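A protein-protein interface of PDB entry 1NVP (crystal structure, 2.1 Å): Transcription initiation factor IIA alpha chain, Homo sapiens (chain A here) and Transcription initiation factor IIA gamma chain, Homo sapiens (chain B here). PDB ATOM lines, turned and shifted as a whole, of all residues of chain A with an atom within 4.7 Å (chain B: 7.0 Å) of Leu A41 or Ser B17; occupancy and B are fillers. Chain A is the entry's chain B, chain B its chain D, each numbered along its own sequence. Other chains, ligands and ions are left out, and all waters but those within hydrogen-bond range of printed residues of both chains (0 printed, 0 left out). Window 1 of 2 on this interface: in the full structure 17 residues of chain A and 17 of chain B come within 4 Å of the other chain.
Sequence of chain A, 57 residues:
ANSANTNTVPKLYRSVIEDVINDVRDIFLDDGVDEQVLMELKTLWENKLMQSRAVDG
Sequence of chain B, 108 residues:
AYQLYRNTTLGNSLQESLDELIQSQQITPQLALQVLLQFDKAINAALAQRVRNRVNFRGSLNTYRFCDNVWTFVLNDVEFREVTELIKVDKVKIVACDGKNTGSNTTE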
ATOM      1  N   ILE A  21      16.826 -10.965  -7.541  1.00  0.00           N
ATOM      2  CA  ILE A  21      16.360 -11.903  -8.559  1.00  0.00           C
ATOM      3  C   ILE A  21      14.994 -11.462  -9.078  1.00  0.00           C
ATOM      4  O   ILE A  21      14.780 -11.378 -10.287  1.00  0.00           O
ATOM      5  CB  ILE A  21      16.276 -13.339  -8.000  1.00  0.00           C
ATOM      6  CG1 ILE A  21      17.676 -13.820  -7.607  1.00  0.00           C
ATOM      7  CG2 ILE A  21      15.680 -14.277  -9.049  1.00  0.00           C
ATOM      8  CD1 ILE A  21      18.684 -13.791  -8.752  1.00  0.00           C
ATOM      9  N   PHE A  28      15.819  -9.412 -17.761  1.00  0.00           N
ATOM     10  CA  PHE A  28      16.250 -10.607 -18.481  1.00  0.00           C
ATOM     11  C   PHE A  28      15.264 -10.861 -19.616  1.00  0.00           C
ATOM     12  O   PHE A  28      15.658 -11.115 -20.759  1.00  0.00           O
ATOM     13  CB  PHE A  28      16.277 -11.821 -17.548  1.00  0.00           C
ATOM     14  CG  PHE A  28      17.583 -12.012 -16.829  1.00  0.00           C
ATOM     15  CD1 PHE A  28      18.250 -13.235 -16.894  1.00  0.00           C
ATOM     16  CD2 PHE A  28      18.145 -10.980 -16.078  1.00  0.00           C
ATOM     17  CE1 PHE A  28      19.456 -13.434 -16.218  1.00  0.00           C
ATOM     18  CE2 PHE A  28      19.351 -11.168 -15.398  1.00  0.00           C
ATOM     19  CZ  PHE A  28      20.008 -12.399 -15.469  1.00  0.00           C
ATOM     20  N   VAL A  37      18.103 -19.055 -17.332  1.00  0.00           N
ATOM     21  CA  VAL A  37      19.379 -18.418 -17.032  1.00  0.00           C
ATOM     22  C   VAL A  37      19.261 -17.654 -15.716  1.00  0.00           C
ATOM     23  O   VAL A  37      20.169 -17.684 -14.887  1.00  0.00           O
ATOM     24  CB  VAL A  37      19.783 -17.441 -18.142  1.00  0.00           C
ATOM     25  CG1 VAL A  37      21.190 -16.894 -17.875  1.00  0.00           C
ATOM     26  CG2 VAL A  37      19.722 -18.141 -19.485  1.00  0.00           C
ATOM     27  N   LEU A  38      18.134 -16.979 -15.515  1.00  0.00           N
ATOM     28  CA  LEU A  38      17.940 -16.233 -14.284  1.00  0.00           C
ATOM     29  C   LEU A  38      18.091 -17.171 -13.094  1.00  0.00           C
ATOM     30  O   LEU A  38      18.791 -16.857 -12.124  1.00  0.00           O
ATOM     31  CB  LEU A  38      16.554 -15.585 -14.249  1.00  0.00           C
ATOM     32  CG  LEU A  38      16.264 -14.757 -12.987  1.00  0.00           C
ATOM     33  CD1 LEU A  38      17.220 -13.573 -12.925  1.00  0.00           C
ATOM     34  CD2 LEU A  38      14.821 -14.269 -12.995  1.00  0.00           C
ATOM     35  N   MET A  39      17.438 -18.328 -13.170  1.00  0.00           N
ATOM     36  CA  MET A  39      17.499 -19.297 -12.083  1.00  0.00           C
ATOM     37  C   MET A  39      18.909 -19.846 -11.897  1.00  0.00           C
ATOM     38  O   MET A  39      19.304 -20.198 -10.786  1.00  0.00           O
ATOM     39  CB  MET A  39      16.517 -20.447 -12.337  1.00  0.00           C
ATOM     40  CG  MET A  39      15.074 -19.997 -12.508  1.00  0.00           C
ATOM     41  SD  MET A  39      14.538 -18.831 -11.231  1.00  0.00           S
ATOM     42  CE  MET A  39      14.332 -19.930  -9.823  1.00  0.00           C
ATOM     43  N   GLU A  40      19.666 -19.934 -12.981  1.00  0.00           N
ATOM     44  CA  GLU A  40      21.029 -20.428 -12.879  1.00  0.00           C
ATOM     45  C   GLU A  40      21.813 -19.387 -12.067  1.00  0.00           C
ATOM     46  O   GLU A  40      22.610 -19.735 -11.193  1.00  0.00           O
ATOM     47  CB  GLU A  40      21.652 -20.592 -14.267  1.00  0.00           C
ATOM     48  CG  GLU A  40      22.792 -21.605 -14.298  1.00  0.00           C
ATOM     49  CD  GLU A  40      23.532 -21.622 -15.621  1.00  0.00           C
ATOM     50  OE1 GLU A  40      22.871 -21.532 -16.678  1.00  0.00           O
ATOM     51  OE2 GLU A  40      24.778 -21.738 -15.603  1.00  0.00           O
ATOM     52  N   LEU A  41      21.564 -18.112 -12.357  1.00  0.00           N
ATOM     53  CA  LEU A  41      22.227 -17.019 -11.644  1.00  0.00           C
ATOM     54  C   LEU A  41      22.002 -17.195 -10.156  1.00  0.00           C
ATOM     55  O   LEU A  41      22.956 -17.297  -9.385  1.00  0.00           O
ATOM     56  CB  LEU A  41      21.663 -15.665 -12.084  1.00  0.00           C
ATOM     57  CG  LEU A  41      22.268 -14.420 -11.425  1.00  0.00           C
ATOM     58  CD1 LEU A  41      23.763 -14.361 -11.725  1.00  0.00           C
ATOM     59  CD2 LEU A  41      21.569 -13.171 -11.953  1.00  0.00           C
ATOM     60  N   LYS A  42      20.737 -17.243  -9.752  1.00  0.00           N
ATOM     61  CA  LYS A  42      20.403 -17.412  -8.345  1.00  0.00           C
ATOM     62  C   LYS A  42      21.119 -18.609  -7.736  1.00  0.00           C
ATOM     63  O   LYS A  42      21.640 -18.526  -6.619  1.00  0.00           O
ATOM     64  CB  LYS A  42      18.897 -17.595  -8.160  1.00  0.00           C
ATOM     65  CG  LYS A  42      18.493 -17.671  -6.696  1.00  0.00           C
ATOM     66  CD  LYS A  42      17.003 -17.880  -6.513  1.00  0.00           C
ATOM     67  CE  LYS A  42      16.560 -17.285  -5.187  1.00  0.00           C
ATOM     68  NZ  LYS A  42      15.392 -17.979  -4.586  1.00  0.00           N
ATOM     69  N   THR A  43      21.138 -19.723  -8.463  1.00  0.00           N
ATOM     70  CA  THR A  43      21.784 -20.936  -7.972  1.00  0.00           C
ATOM     71  C   THR A  43      23.290 -20.742  -7.834  1.00  0.00           C
ATOM     72  O   THR A  43      23.864 -21.058  -6.794  1.00  0.00           O
ATOM     73  CB  THR A  43      21.510 -22.141  -8.906  1.00  0.00           C
ATOM     74  OG1 THR A  43      20.101 -22.393  -8.953  1.00  0.00           O
ATOM     75  CG2 THR A  43      22.216 -23.388  -8.394  1.00  0.00           C
ATOM     76  N   LEU A  44      23.926 -20.236  -8.889  1.00  0.00           N
ATOM     77  CA  LEU A  44      25.365 -19.983  -8.864  1.00  0.00           C
ATOM     78  C   LEU A  44      25.688 -19.093  -7.668  1.00  0.00           C
ATOM     79  O   LEU A  44      26.592 -19.377  -6.880  1.00  0.00           O
ATOM     80  CB  LEU A  44      25.808 -19.267 -10.142  1.00  0.00           C
ATOM     81  CG  LEU A  44      25.885 -20.050 -11.452  1.00  0.00           C
ATOM     82  CD1 LEU A  44      26.236 -19.106 -12.592  1.00  0.00           C
ATOM     83  CD2 LEU A  44      26.935 -21.144 -11.328  1.00  0.00           C
ATOM     84  N   TRP A  45      24.916 -18.019  -7.543  1.00  0.00           N
ATOM     85  CA  TRP A  45      25.074 -17.040  -6.480  1.00  0.00           C
ATOM     86  C   TRP A  45      24.904 -17.614  -5.075  1.00  0.00           C
ATOM     87  O   TRP A  45      25.769 -17.426  -4.216  1.00  0.00           O
ATOM     88  CB  TRP A  45      24.080 -15.896  -6.701  1.00  0.00           C
ATOM     89  CG  TRP A  45      24.299 -14.700  -5.821  1.00  0.00           C
ATOM     90  CD1 TRP A  45      25.331 -14.494  -4.943  1.00  0.00           C
ATOM     91  CD2 TRP A  45      23.473 -13.532  -5.747  1.00  0.00           C
ATOM     92  NE1 TRP A  45      25.196 -13.270  -4.329  1.00  0.00           N
ATOM     93  CE2 TRP A  45      24.064 -12.658  -4.804  1.00  0.00           C
ATOM     94  CE3 TRP A  45      22.289 -13.137  -6.387  1.00  0.00           C
ATOM     95  CZ2 TRP A  45      23.513 -11.411  -4.486  1.00  0.00           C
ATOM     96  CZ3 TRP A  45      21.737 -11.897  -6.071  1.00  0.00           C
ATOM     97  CH2 TRP A  45      22.352 -11.049  -5.126  1.00  0.00           C
ATOM     98  N   LYS A  48      27.709 -20.041  -4.183  1.00  0.00           N
ATOM     99  CA  LYS A  48      28.997 -19.419  -3.945  1.00  0.00           C
ATOM    100  C   LYS A  48      29.053 -18.891  -2.523  1.00  0.00           C
ATOM    101  O   LYS A  48      30.118 -18.873  -1.905  1.00  0.00           O
ATOM    102  CB  LYS A  48      29.268 -18.326  -4.975  1.00  0.00           C
ATOM    103  CG  LYS A  48      30.238 -18.835  -6.015  1.00  0.00           C
ATOM    104  CD  LYS A  48      30.153 -18.151  -7.355  1.00  0.00           C
ATOM    105  CE  LYS A  48      30.895 -19.006  -8.375  1.00  0.00           C
ATOM    106  NZ  LYS A  48      31.122 -18.326  -9.672  1.00  0.00           N
ATOM    107  N   ASN B  12      30.656 -10.068  -4.215  1.00  0.00           N
ATOM    108  CA  ASN B  12      31.628 -10.755  -5.061  1.00  0.00           C
ATOM    109  C   ASN B  12      31.091 -12.076  -5.602  1.00  0.00           C
ATOM    110  O   ASN B  12      31.316 -12.416  -6.766  1.00  0.00           O
ATOM    111  CB  ASN B  12      32.939 -10.995  -4.302  1.00  0.00           C
ATOM    112  CG  ASN B  12      33.811  -9.751  -4.241  1.00  0.00           C
ATOM    113  OD1 ASN B  12      34.134  -9.153  -5.270  1.00  0.00           O
ATOM    114  ND2 ASN B  12      34.195  -9.358  -3.033  1.00  0.00           N
ATOM    115  N   SER B  13      30.391 -12.827  -4.762  1.00  0.00           N
ATOM    116  CA  SER B  13      29.823 -14.086  -5.219  1.00  0.00           C
ATOM    117  C   SER B  13      28.917 -13.767  -6.411  1.00  0.00           C
ATOM    118  O   SER B  13      28.878 -14.505  -7.400  1.00  0.00           O
ATOM    119  CB  SER B  13      29.040 -14.755  -4.088  1.00  0.00           C
ATOM    120  OG  SER B  13      28.132 -13.857  -3.482  1.00  0.00           O
ATOM    121  N   LEU B  14      28.222 -12.636  -6.331  1.00  0.00           N
ATOM    122  CA  LEU B  14      27.338 -12.208  -7.411  1.00  0.00           C
ATOM    123  C   LEU B  14      28.110 -11.939  -8.702  1.00  0.00           C
ATOM    124  O   LEU B  14      27.764 -12.457  -9.766  1.00  0.00           O
ATOM    125  CB  LEU B  14      26.570 -10.949  -6.989  1.00  0.00           C
ATOM    126  CG  LEU B  14      25.689 -10.257  -8.036  1.00  0.00           C
ATOM    127  CD1 LEU B  14      24.691 -11.247  -8.630  1.00  0.00           C
ATOM    128  CD2 LEU B  14      24.962  -9.091  -7.385  1.00  0.00           C
ATOM    129  N   GLN B  15      29.164 -11.131  -8.607  1.00  0.00           N
ATOM    130  CA  GLN B  15      29.968 -10.792  -9.776  1.00  0.00           C
ATOM    131  C   GLN B  15      30.585 -12.015 -10.430  1.00  0.00           C
ATOM    132  O   GLN B  15      30.659 -12.107 -11.657  1.00  0.00           O
ATOM    133  CB  GLN B  15      31.088  -9.820  -9.393  1.00  0.00           C
ATOM    134  CG  GLN B  15      30.603  -8.509  -8.809  1.00  0.00           C
ATOM    135  CD  GLN B  15      31.667  -7.434  -8.849  1.00  0.00           C
ATOM    136  OE1 GLN B  15      32.180  -7.096  -9.916  1.00  0.00           O
ATOM    137  NE2 GLN B  15      32.004  -6.889  -7.686  1.00  0.00           N
ATOM    138  N   GLU B  16      31.048 -12.943  -9.602  1.00  0.00           N
ATOM    139  CA  GLU B  16      31.668 -14.160 -10.100  1.00  0.00           C
ATOM    140  C   GLU B  16      30.631 -14.957 -10.875  1.00  0.00           C
ATOM    141  O   GLU B  16      30.899 -15.444 -11.976  1.00  0.00           O
ATOM    142  CB  GLU B  16      32.219 -14.973  -8.928  1.00  0.00           C
ATOM    143  CG  GLU B  16      33.345 -14.255  -8.192  1.00  0.00           C
ATOM    144  CD  GLU B  16      33.586 -14.798  -6.800  1.00  0.00           C
ATOM    145  OE1 GLU B  16      32.997 -15.844  -6.452  1.00  0.00           O
ATOM    146  OE2 GLU B  16      34.371 -14.177  -6.053  1.00  0.00           O
ATOM    147  N   SER B  17      29.441 -15.070 -10.296  1.00  0.00           N
ATOM    148  CA  SER B  17      28.354 -15.791 -10.937  1.00  0.00           C
ATOM    149  C   SER B  17      28.054 -15.140 -12.282  1.00  0.00           C
ATOM    150  O   SER B  17      27.860 -15.829 -13.286  1.00  0.00           O
ATOM    151  CB  SER B  17      27.108 -15.758 -10.056  1.00  0.00           C
ATOM    152  OG  SER B  17      27.377 -16.294  -8.772  1.00  0.00           O
ATOM    153  N   LEU B  18      28.031 -13.808 -12.304  1.00  0.00           N
ATOM    154  CA  LEU B  18      27.752 -13.073 -13.534  1.00  0.00           C
ATOM    155  C   LEU B  18      28.822 -13.284 -14.599  1.00  0.00           C
ATOM    156  O   LEU B  18      28.509 -13.498 -15.773  1.00  0.00           O
ATOM    157  CB  LEU B  18      27.607 -11.577 -13.240  1.00  0.00           C
ATOM    158  CG  LEU B  18      26.372 -11.129 -12.452  1.00  0.00           C
ATOM    159  CD1 LEU B  18      26.486  -9.650 -12.108  1.00  0.00           C
ATOM    160  CD2 LEU B  18      25.116 -11.384 -13.278  1.00  0.00           C
ATOM    161  N   ASP B  19      30.087 -13.224 -14.193  1.00  0.00           N
ATOM    162  CA  ASP B  19      31.185 -13.410 -15.134  1.00  0.00           C
ATOM    163  C   ASP B  19      31.100 -14.757 -15.836  1.00  0.00           C
ATOM    164  O   ASP B  19      31.375 -14.854 -17.033  1.00  0.00           O
ATOM    165  CB  ASP B  19      32.532 -13.274 -14.422  1.00  0.00           C
ATOM    166  CG  ASP B  19      32.838 -11.844 -14.040  1.00  0.00           C
ATOM    167  OD1 ASP B  19      32.805 -10.971 -14.937  1.00  0.00           O
ATOM    168  OD2 ASP B  19      33.111 -11.592 -12.847  1.00  0.00           O
ATOM    169  N   GLU B  20      30.729 -15.794 -15.090  1.00  0.00           N
ATOM    170  CA  GLU B  20      30.586 -17.121 -15.675  1.00  0.00           C
ATOM    171  C   GLU B  20      29.572 -17.022 -16.807  1.00  0.00           C
ATOM    172  O   GLU B  20      29.871 -17.324 -17.962  1.00  0.00           O
ATOM    173  CB  GLU B  20      30.074 -18.118 -14.638  1.00  0.00           C
ATOM    174  CG  GLU B  20      31.079 -18.523 -13.581  1.00  0.00           C
ATOM    175  CD  GLU B  20      30.656 -19.789 -12.862  1.00  0.00           C
ATOM    176  OE1 GLU B  20      30.407 -20.802 -13.552  1.00  0.00           O
ATOM    177  OE2 GLU B  20      30.571 -19.780 -11.617  1.00  0.00           O
ATOM    178  N   LEU B  21      28.367 -16.583 -16.455  1.00  0.00           N
ATOM    179  CA  LEU B  21      27.288 -16.431 -17.419  1.00  0.00           C
ATOM    180  C   LEU B  21      27.724 -15.572 -18.595  1.00  0.00           C
ATOM    181  O   LEU B  21      27.234 -15.740 -19.710  1.00  0.00           O
ATOM    182  CB  LEU B  21      26.062 -15.827 -16.733  1.00  0.00           C
ATOM    183  CG  LEU B  21      25.508 -16.735 -15.629  1.00  0.00           C
ATOM    184  CD1 LEU B  21      24.353 -16.051 -14.910  1.00  0.00           C
ATOM    185  CD2 LEU B  21      25.057 -18.061 -16.242  1.00  0.00           C
ATOM    186  N   ILE B  22      28.646 -14.649 -18.350  1.00  0.00           N
ATOM    187  CA  ILE B  22      29.144 -13.799 -19.421  1.00  0.00           C
ATOM    188  C   ILE B  22      30.120 -14.636 -20.233  1.00  0.00           C
ATOM    189  O   ILE B  22      30.124 -14.603 -21.463  1.00  0.00           O
ATOM    190  CB  ILE B  22      29.889 -12.570 -18.864  1.00  0.00           C
ATOM    191  CG1 ILE B  22      28.916 -11.681 -18.089  1.00  0.00           C
ATOM    192  CG2 ILE B  22      30.540 -11.795 -20.003  1.00  0.00           C
ATOM    193  CD1 ILE B  22      29.591 -10.701 -17.157  1.00  0.00           C
ATOM    194  N   GLN B  23      30.937 -15.400 -19.519  1.00  0.00           N
ATOM    195  CA  GLN B  23      31.942 -16.252 -20.137  1.00  0.00           C
ATOM    196  C   GLN B  23      31.288 -17.277 -21.062  1.00  0.00           C
ATOM    197  O   GLN B  23      31.706 -17.440 -22.210  1.00  0.00           O
ATOM    198  CB  GLN B  23      32.766 -16.946 -19.044  1.00  0.00           C
ATOM    199  CG  GLN B  23      34.179 -17.314 -19.473  1.00  0.00           C
ATOM    200  CD  GLN B  23      34.295 -18.740 -19.973  1.00  0.00           C
ATOM    201  OE1 GLN B  23      34.423 -19.677 -19.184  1.00  0.00           O
ATOM    202  NE2 GLN B  23      34.240 -18.914 -21.290  1.00  0.00           N
ATOM    203  N   ILE B  27      24.662 -14.372 -20.863  1.00  0.00           N
ATOM    204  CA  ILE B  27      24.173 -13.019 -20.615  1.00  0.00           C
ATOM    205  C   ILE B  27      25.219 -12.049 -21.149  1.00  0.00           C
ATOM    206  O   ILE B  27      26.388 -12.410 -21.283  1.00  0.00           O
ATOM    207  CB  ILE B  27      23.965 -12.741 -19.109  1.00  0.00           C
ATOM    208  CG1 ILE B  27      25.315 -12.692 -18.389  1.00  0.00           C
ATOM    209  CG2 ILE B  27      23.085 -13.819 -18.498  1.00  0.00           C
ATOM    210  CD1 ILE B  27      25.200 -12.357 -16.917  1.00  0.00           C
ATOM    211  N   VAL B  35      22.344  -5.889 -13.464  1.00  0.00           N
ATOM    212  CA  VAL B  35      22.070  -6.700 -12.282  1.00  0.00           C
ATOM    213  C   VAL B  35      22.800  -6.124 -11.068  1.00  0.00           C
ATOM    214  O   VAL B  35      22.247  -6.057  -9.965  1.00  0.00           O
ATOM    215  CB  VAL B  35      22.543  -8.151 -12.474  1.00  0.00           C
ATOM    216  CG1 VAL B  35      22.235  -8.960 -11.223  1.00  0.00           C
ATOM    217  CG2 VAL B  35      21.883  -8.757 -13.699  1.00  0.00           C
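OG of Ser B17 sits at hydrogen-bond distance from O of Ser B13.
The backbone NH (N) of Ile B27 sits at hydrogen-bond distance from the backbone carbonyl oxygen (O) of Leu B21 (3.1 Å).
NE1 of Trp A45 is in hydrogen-bond range of OG of Ser B13.
N of Trp A45 lies within hydrogen-bond range of OG of Ser B17 (3.2 Å).
The side-chain carboxylate (OE2) of Glu B20 lies within salt-bridge range of the side-chain amino group (NZ) of Lys A48.
Of the printed residues of chain B, Leu A41 touches Ser B17 (3.99 Å), Leu B18 (3.6 Å) and Leu B21 (3.7 Å).
Of the printed residues of chain B, Lys A48 touches Ser B13 (3.7 Å), Glu B16 (3.6 Å), Ser B17 (3.6 Å) and Glu B20 (2.5 Å).
Printed residues of chain A within 4 Å of Glu B16: Lys A48.
Of the printed residues of chain A, Ser B17 touches Leu A41 (3.99 Å), Leu A44 (3.5 Å), Trp A45 (3.2 Å) and Lys A48 (3.6 Å).
Of the printed residues of chain A, Leu B21 touches Glu A40 (3.7 Å), Leu A41 (3.7 Å) and Leu A44 (3.9 Å).
Of the printed residues of chain A, Ile B27 touches Val A37 (3.7 Å).
The nearest printed residue of chain B that does not touch Leu A41 is Val B35 (4.3 Å).
The nearest printed residue of chain A that does not touch Ser B17 is Glu A40 (6.1 Å).
Hydrophobic or aromatic side chains of chain A that line the printed part of chain B: Phe A28, Val A37, Leu A41, Leu A44 and Trp A45.
Printed residues of chain B that touch a printed residue of chain A: Ser B13, Leu B14, Glu B16, Ser B17, Leu B18, Glu B20, Leu B21, Ile B27 and Val B35.
Hydrophobic or aromatic side chains of chain B within 4 Å of the printed part of chain A: Leu B14, Leu B18, Leu B21, Ile B27 and Val B35.
Among the printed residues, 16 pairs touch across the chains.
Among the printed residues, Asp or Glu carboxylates within 4 Å of a Lys or Arg side-chain nitrogen of the other chain: Lys A48 with Glu B20.
Val A37 touches Ile B27 (CG1 to CG2, 3.7 Å).
Leu B21 touches Glu A40.
Leu A41 touches Leu B18.
CD1 of Leu A41 touches CD1 of Leu B21, at 3.7 Å.
C of Leu A44 touches OG of Ser B17 (3.5 Å).
OE2 of Glu B20 touches CD2 of Leu A44, 3.9 Å away.
Leu A44 touches Leu B21 (CD1 to CG, 3.9 Å).
NE1 of Trp A45 touches N of Leu B14, at 3.7 Å.
Lys A48 touches Ser B13.
Glu B16 touches Lys A48 (CB to NZ, 3.6 Å).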
